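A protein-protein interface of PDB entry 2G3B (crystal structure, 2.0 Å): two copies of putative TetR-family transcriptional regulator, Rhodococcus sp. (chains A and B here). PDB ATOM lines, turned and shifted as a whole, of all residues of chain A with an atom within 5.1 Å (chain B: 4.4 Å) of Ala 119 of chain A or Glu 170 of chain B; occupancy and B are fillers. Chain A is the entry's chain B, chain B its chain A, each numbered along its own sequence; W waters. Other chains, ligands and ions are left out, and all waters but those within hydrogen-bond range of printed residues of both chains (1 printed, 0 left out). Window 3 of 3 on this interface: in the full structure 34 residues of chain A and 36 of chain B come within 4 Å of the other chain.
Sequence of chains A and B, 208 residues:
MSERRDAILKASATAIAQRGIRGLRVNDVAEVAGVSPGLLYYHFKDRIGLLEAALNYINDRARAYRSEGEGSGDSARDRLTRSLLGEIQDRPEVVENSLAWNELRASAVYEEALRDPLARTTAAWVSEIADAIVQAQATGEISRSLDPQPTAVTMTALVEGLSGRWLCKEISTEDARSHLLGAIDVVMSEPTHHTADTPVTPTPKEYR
Water W1 bridges the side-chain carboxylate of Glu 170 of chain B (2.6 Å) and the backbone carbonyl oxygen of Arg 115 of chain A (2.8 Å).
OE1 of Glu 170 of chain B lies within salt-bridge range of NH1 of Arg 105 of chain A, at 2.9 Å. The backbone carbonyl oxygen (O) of Arg 105 of chain A is in hydrogen-bond range of the side-chain sulfur (SG) of Cys 168 of chain B (3.5 Å).
OG1 of Thr 121 of chain A is in hydrogen-bond range of O of Leu 118 of chain A (3.2 Å). The backbone carbonyl oxygen (O) of Leu 118 of chain A sits at hydrogen-bond distance from the side-chain hydroxyl (OG1) of Thr 122 of chain A, at 2.7 Å. The guanidinium group (NE) of Arg 165 of chain B lies within salt-bridge range of the side-chain carboxylate (OE2) of Glu 170 of chain B, at 3.9 Å. The guanidinium group of Arg 105 of chain A lies within hydrogen-bond range of the side-chain hydroxyl of Thr 122 of chain A, at 3.3 Å.
No position is printed for both chains.
Among the printed residues, merely in contact across the chains: Arg 105 of chain A with Arg 165 of chain B, Arg 115 of chain A with Cys 168 of chain B, Arg 115 of chain A with Lys 169 of chain B, Leu 118 of chain A with Glu 170 of chain B, Ala 119 of chain A with Glu 170 of chain B, Thr 122 of chain A with Arg 165 of chain B and Thr 122 of chain A with Glu 170 of chain B.
Of the printed residues of chain B, Arg 115 of chain A touches Cys 168 and Lys 169. Of the printed residues of chain B, Leu 118 of chain A touches Glu 170 (3.9 Å). Printed residues of chain B within 4 Å of Thr 122 of chain A: Arg 165 (3.7 Å) and Glu 170 (3.4 Å). Ala 123 of chain A touches none of the printed residues of chain B. Printed residues of chain A within 4 Å of Cys 168 of chain B: Arg 105 (3.5 Å) and Arg 115 (3.3 Å). Printed residues of chain A within 4 Å of Lys 169 of chain B: Arg 115. Printed residues of chain A within 4 Å of Glu 170 of chain B: Arg 105 (2.9 Å), Leu 118 (3.9 Å), Ala 119 (3.6 Å) and Thr 122 (3.4 Å). The nearest residue of chain A that does not touch Glu 170 of chain B is Arg 115 of chain A (4.6 Å).
Of the 5 printed residues of chain B, 4 touch a printed residue of chain A. Printed residues of chain B that touch a printed residue of chain A: Arg 165, Cys 168, Lys 169 and Glu 170. Among the printed residues, 9 pairs touch across the chains. Among the printed residues, Asp or Glu carboxylates within 4 Å of a Lys or Arg side-chain nitrogen of the other chain: Arg 105 of chain A with Glu 170 of chain B (2.9 Å).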
ATOM      1  N   ARG A 105     -25.080  -2.594 -21.943  1.00  0.00           N
ATOM      2  CA  ARG A 105     -24.179  -3.742 -21.620  1.00  0.00           C
ATOM      3  C   ARG A 105     -24.898  -4.901 -20.955  1.00  0.00           C
ATOM      4  O   ARG A 105     -24.691  -6.082 -21.311  1.00  0.00           O
ATOM      5  CB  ARG A 105     -23.010  -3.254 -20.716  1.00  0.00           C
ATOM      6  CG  ARG A 105     -22.264  -4.393 -19.970  1.00  0.00           C
ATOM      7  CD  ARG A 105     -21.573  -5.402 -20.920  1.00  0.00           C
ATOM      8  NE  ARG A 105     -20.416  -4.751 -21.556  1.00  0.00           N
ATOM      9  CZ  ARG A 105     -19.767  -5.205 -22.620  1.00  0.00           C
ATOM     10  NH1 ARG A 105     -20.132  -6.322 -23.250  1.00  0.00           N
ATOM     11  NH2 ARG A 105     -18.745  -4.498 -23.072  1.00  0.00           N
ATOM     12  N   LEU A 114     -27.534  -6.676 -30.233  1.00  0.00           N
ATOM     13  CA  LEU A 114     -26.718  -5.560 -29.709  1.00  0.00           C
ATOM     14  C   LEU A 114     -25.249  -5.959 -29.412  1.00  0.00           C
ATOM     15  O   LEU A 114     -24.377  -5.097 -29.178  1.00  0.00           O
ATOM     16  CB  LEU A 114     -27.362  -4.983 -28.468  1.00  0.00           C
ATOM     17  CG  LEU A 114     -28.667  -4.197 -28.731  1.00  0.00           C
ATOM     18  CD1 LEU A 114     -29.171  -3.819 -27.347  1.00  0.00           C
ATOM     19  CD2 LEU A 114     -28.484  -2.938 -29.659  1.00  0.00           C
ATOM     20  N   ARG A 115     -24.952  -7.258 -29.501  1.00  0.00           N
ATOM     21  CA  ARG A 115     -23.613  -7.739 -29.109  1.00  0.00           C
ATOM     22  C   ARG A 115     -22.544  -7.234 -30.074  1.00  0.00           C
ATOM     23  O   ARG A 115     -21.506  -6.723 -29.635  1.00  0.00           O
ATOM     24  CB  ARG A 115     -23.617  -9.272 -29.048  1.00  0.00           C
ATOM     25  CG  ARG A 115     -24.451  -9.781 -27.940  1.00  0.00           C
ATOM     26  CD  ARG A 115     -24.519 -11.320 -28.022  1.00  0.00           C
ATOM     27  NE  ARG A 115     -25.248 -11.882 -26.893  1.00  0.00           N
ATOM     28  CZ  ARG A 115     -25.368 -13.187 -26.686  1.00  0.00           C
ATOM     29  NH1 ARG A 115     -24.840 -14.044 -27.575  1.00  0.00           N
ATOM     30  NH2 ARG A 115     -26.025 -13.635 -25.618  1.00  0.00           N
ATOM     31  N   ASP A 116     -22.787  -7.322 -31.391  1.00  0.00           N
ATOM     32  CA  ASP A 116     -21.753  -6.867 -32.358  1.00  0.00           C
ATOM     33  C   ASP A 116     -21.389  -5.350 -32.191  1.00  0.00           C
ATOM     34  O   ASP A 116     -20.185  -4.981 -32.086  1.00  0.00           O
ATOM     35  CB  ASP A 116     -22.179  -7.207 -33.826  1.00  0.00           C
ATOM     36  CG  ASP A 116     -21.254  -6.541 -34.877  1.00  0.00           C
ATOM     37  OD1 ASP A 116     -20.225  -7.146 -35.247  1.00  0.00           O
ATOM     38  OD2 ASP A 116     -21.537  -5.400 -35.340  1.00  0.00           O
ATOM     39  N   PRO A 117     -22.400  -4.459 -32.189  1.00  0.00           N
ATOM     40  CA  PRO A 117     -22.006  -3.020 -32.025  1.00  0.00           C
ATOM     41  C   PRO A 117     -21.327  -2.748 -30.674  1.00  0.00           C
ATOM     42  O   PRO A 117     -20.360  -1.952 -30.587  1.00  0.00           O
ATOM     43  CB  PRO A 117     -23.340  -2.243 -32.132  1.00  0.00           C
ATOM     44  CG  PRO A 117     -24.440  -3.276 -32.075  1.00  0.00           C
ATOM     45  CD  PRO A 117     -23.840  -4.633 -32.454  1.00  0.00           C
ATOM     46  N   LEU A 118     -21.780  -3.446 -29.642  1.00  0.00           N
ATOM     47  CA  LEU A 118     -21.135  -3.331 -28.317  1.00  0.00           C
ATOM     48  C   LEU A 118     -19.697  -3.832 -28.308  1.00  0.00           C
ATOM     49  O   LEU A 118     -18.830  -3.177 -27.704  1.00  0.00           O
ATOM     50  CB  LEU A 118     -21.989  -3.995 -27.243  1.00  0.00           C
ATOM     51  CG  LEU A 118     -21.646  -3.943 -25.770  1.00  0.00           C
ATOM     52  CD1 LEU A 118     -21.743  -2.480 -25.293  1.00  0.00           C
ATOM     53  CD2 LEU A 118     -22.696  -4.759 -24.996  1.00  0.00           C
ATOM     54  N   ALA A 119     -19.445  -4.954 -28.978  1.00  0.00           N
ATOM     55  CA  ALA A 119     -18.105  -5.534 -29.078  1.00  0.00           C
ATOM     56  C   ALA A 119     -17.175  -4.544 -29.847  1.00  0.00           C
ATOM     57  O   ALA A 119     -16.083  -4.244 -29.394  1.00  0.00           O
ATOM     58  CB  ALA A 119     -18.163  -6.927 -29.813  1.00  0.00           C
ATOM     59  N   ARG A 120     -17.640  -4.032 -30.984  1.00  0.00           N
ATOM     60  CA  ARG A 120     -16.806  -3.155 -31.810  1.00  0.00           C
ATOM     61  C   ARG A 120     -16.485  -1.820 -31.114  1.00  0.00           C
ATOM     62  O   ARG A 120     -15.355  -1.314 -31.164  1.00  0.00           O
ATOM     63  CB  ARG A 120     -17.491  -2.866 -33.131  1.00  0.00           C
ATOM     64  CG  ARG A 120     -17.448  -4.003 -34.127  1.00  0.00           C
ATOM     65  CD  ARG A 120     -17.891  -3.431 -35.460  1.00  0.00           C
ATOM     66  NE  ARG A 120     -19.347  -3.432 -35.591  1.00  0.00           N
ATOM     67  CZ  ARG A 120     -20.160  -2.406 -35.399  1.00  0.00           C
ATOM     68  NH1 ARG A 120     -19.706  -1.181 -35.031  1.00  0.00           N
ATOM     69  NH2 ARG A 120     -21.462  -2.627 -35.571  1.00  0.00           N
ATOM     70  N   THR A 121     -17.483  -1.195 -30.512  1.00  0.00           N
ATOM     71  CA  THR A 121     -17.231   0.055 -29.810  1.00  0.00           C
ATOM     72  C   THR A 121     -16.390  -0.250 -28.569  1.00  0.00           C
ATOM     73  O   THR A 121     -15.552   0.524 -28.194  1.00  0.00           O
ATOM     74  CB  THR A 121     -18.542   0.753 -29.347  1.00  0.00           C
ATOM     75  OG1 THR A 121     -19.327  -0.173 -28.597  1.00  0.00           O
ATOM     76  CG2 THR A 121     -19.361   1.242 -30.518  1.00  0.00           C
ATOM     77  N   THR A 122     -16.630  -1.363 -27.879  1.00  0.00           N
ATOM     78  CA  THR A 122     -15.758  -1.670 -26.738  1.00  0.00           C
ATOM     79  C   THR A 122     -14.322  -1.949 -27.233  1.00  0.00           C
ATOM     80  O   THR A 122     -13.339  -1.590 -26.530  1.00  0.00           O
ATOM     81  CB  THR A 122     -16.314  -2.867 -25.911  1.00  0.00           C
ATOM     82  OG1 THR A 122     -17.614  -2.488 -25.426  1.00  0.00           O
ATOM     83  CG2 THR A 122     -15.396  -3.219 -24.671  1.00  0.00           C
ATOM     84  N   ALA A 123     -14.189  -2.583 -28.399  1.00  0.00           N
ATOM     85  CA  ALA A 123     -12.837  -2.895 -28.953  1.00  0.00           C
ATOM     86  C   ALA A 123     -12.044  -1.614 -29.157  1.00  0.00           C
ATOM     87  O   ALA A 123     -10.819  -1.608 -28.967  1.00  0.00           O
ATOM     88  CB  ALA A 123     -12.878  -3.669 -30.318  1.00  0.00           C
ATOM     89  N   ALA A 124     -12.747  -0.556 -29.551  1.00  0.00           N
ATOM     90  CA  ALA A 124     -12.151   0.753 -29.808  1.00  0.00           C
ATOM     91  C   ALA A 124     -11.667   1.445 -28.525  1.00  0.00           C
ATOM     92  O   ALA A 124     -10.651   2.159 -28.538  1.00  0.00           O
ATOM     93  CB  ALA A 124     -13.172   1.642 -30.608  1.00  0.00           C
ATOM     94  N   ARG B 165     -19.040  -8.981 -19.806  1.00  0.00           N
ATOM     95  CA  ARG B 165     -18.614  -9.216 -21.192  1.00  0.00           C
ATOM     96  C   ARG B 165     -18.712 -10.686 -21.585  1.00  0.00           C
ATOM     97  O   ARG B 165     -19.080 -11.045 -22.712  1.00  0.00           O
ATOM     98  CB  ARG B 165     -17.151  -8.756 -21.304  1.00  0.00           C
ATOM     99  CG  ARG B 165     -17.019  -7.210 -21.203  1.00  0.00           C
ATOM    100  CD  ARG B 165     -15.681  -6.774 -21.793  1.00  0.00           C
ATOM    101  NE  ARG B 165     -15.480  -5.330 -21.499  1.00  0.00           N
ATOM    102  CZ  ARG B 165     -14.288  -4.757 -21.412  1.00  0.00           C
ATOM    103  NH1 ARG B 165     -13.198  -5.520 -21.570  1.00  0.00           N
ATOM    104  NH2 ARG B 165     -14.197  -3.441 -21.171  1.00  0.00           N
ATOM    105  N   CYS B 168     -22.218 -11.736 -22.568  1.00  0.00           N
ATOM    106  CA  CYS B 168     -22.543 -11.236 -23.919  1.00  0.00           C
ATOM    107  C   CYS B 168     -21.769 -11.967 -25.023  1.00  0.00           C
ATOM    108  O   CYS B 168     -21.744 -11.520 -26.185  1.00  0.00           O
ATOM    109  CB  CYS B 168     -22.069  -9.747 -24.041  1.00  0.00           C
ATOM    110  SG  CYS B 168     -22.944  -8.625 -23.036  1.00  0.00           S
ATOM    111  N   LYS B 169     -21.020 -13.010 -24.645  1.00  0.00           N
ATOM    112  CA  LYS B 169     -20.068 -13.713 -25.510  1.00  0.00           C
ATOM    113  C   LYS B 169     -19.013 -12.833 -26.142  1.00  0.00           C
ATOM    114  O   LYS B 169     -18.507 -13.157 -27.204  1.00  0.00           O
ATOM    115  CB  LYS B 169     -20.798 -14.500 -26.619  1.00  0.00           C
ATOM    116  CG  LYS B 169     -21.975 -15.347 -26.111  1.00  0.00           C
ATOM    117  CD  LYS B 169     -21.485 -16.673 -25.581  1.00  0.00           C
ATOM    118  CE  LYS B 169     -22.646 -17.630 -25.267  1.00  0.00           C
ATOM    119  NZ  LYS B 169     -22.907 -18.702 -26.348  1.00  0.00           N
ATOM    120  N   GLU B 170     -18.693 -11.723 -25.488  1.00  0.00           N
ATOM    121  CA  GLU B 170     -17.702 -10.752 -26.001  1.00  0.00           C
ATOM    122  C   GLU B 170     -16.251 -11.172 -25.683  1.00  0.00           C
ATOM    123  O   GLU B 170     -15.288 -10.746 -26.346  1.00  0.00           O
ATOM    124  CB  GLU B 170     -17.966  -9.387 -25.353  1.00  0.00           C
ATOM    125  CG  GLU B 170     -17.197  -8.284 -25.973  1.00  0.00           C
ATOM    126  CD  GLU B 170     -17.739  -6.972 -25.556  1.00  0.00           C
ATOM    127  OE1 GLU B 170     -18.924  -6.673 -25.814  1.00  0.00           O
ATOM    128  OE2 GLU B 170     -16.975  -6.204 -24.992  1.00  0.00           O
ATOM    129  N   ILE B 171     -16.109 -11.962 -24.621  1.00  0.00           N
ATOM    130  CA  ILE B 171     -14.845 -12.503 -24.242  1.00  0.00           C
ATOM    131  C   ILE B 171     -15.087 -13.991 -23.915  1.00  0.00           C
ATOM    132  O   ILE B 171     -16.152 -14.339 -23.352  1.00  0.00           O
ATOM    133  CB  ILE B 171     -14.274 -11.705 -23.012  1.00  0.00           C
ATOM    134  CG1 ILE B 171     -12.810 -12.132 -22.788  1.00  0.00           C
ATOM    135  CG2 ILE B 171     -15.183 -11.915 -21.794  1.00  0.00           C
ATOM    136  CD1 ILE B 171     -12.031 -11.428 -21.649  1.00  0.00           C
HETATM  137  O   HOH W   1     -20.817  -7.908 -27.141  1.00  0.00           O
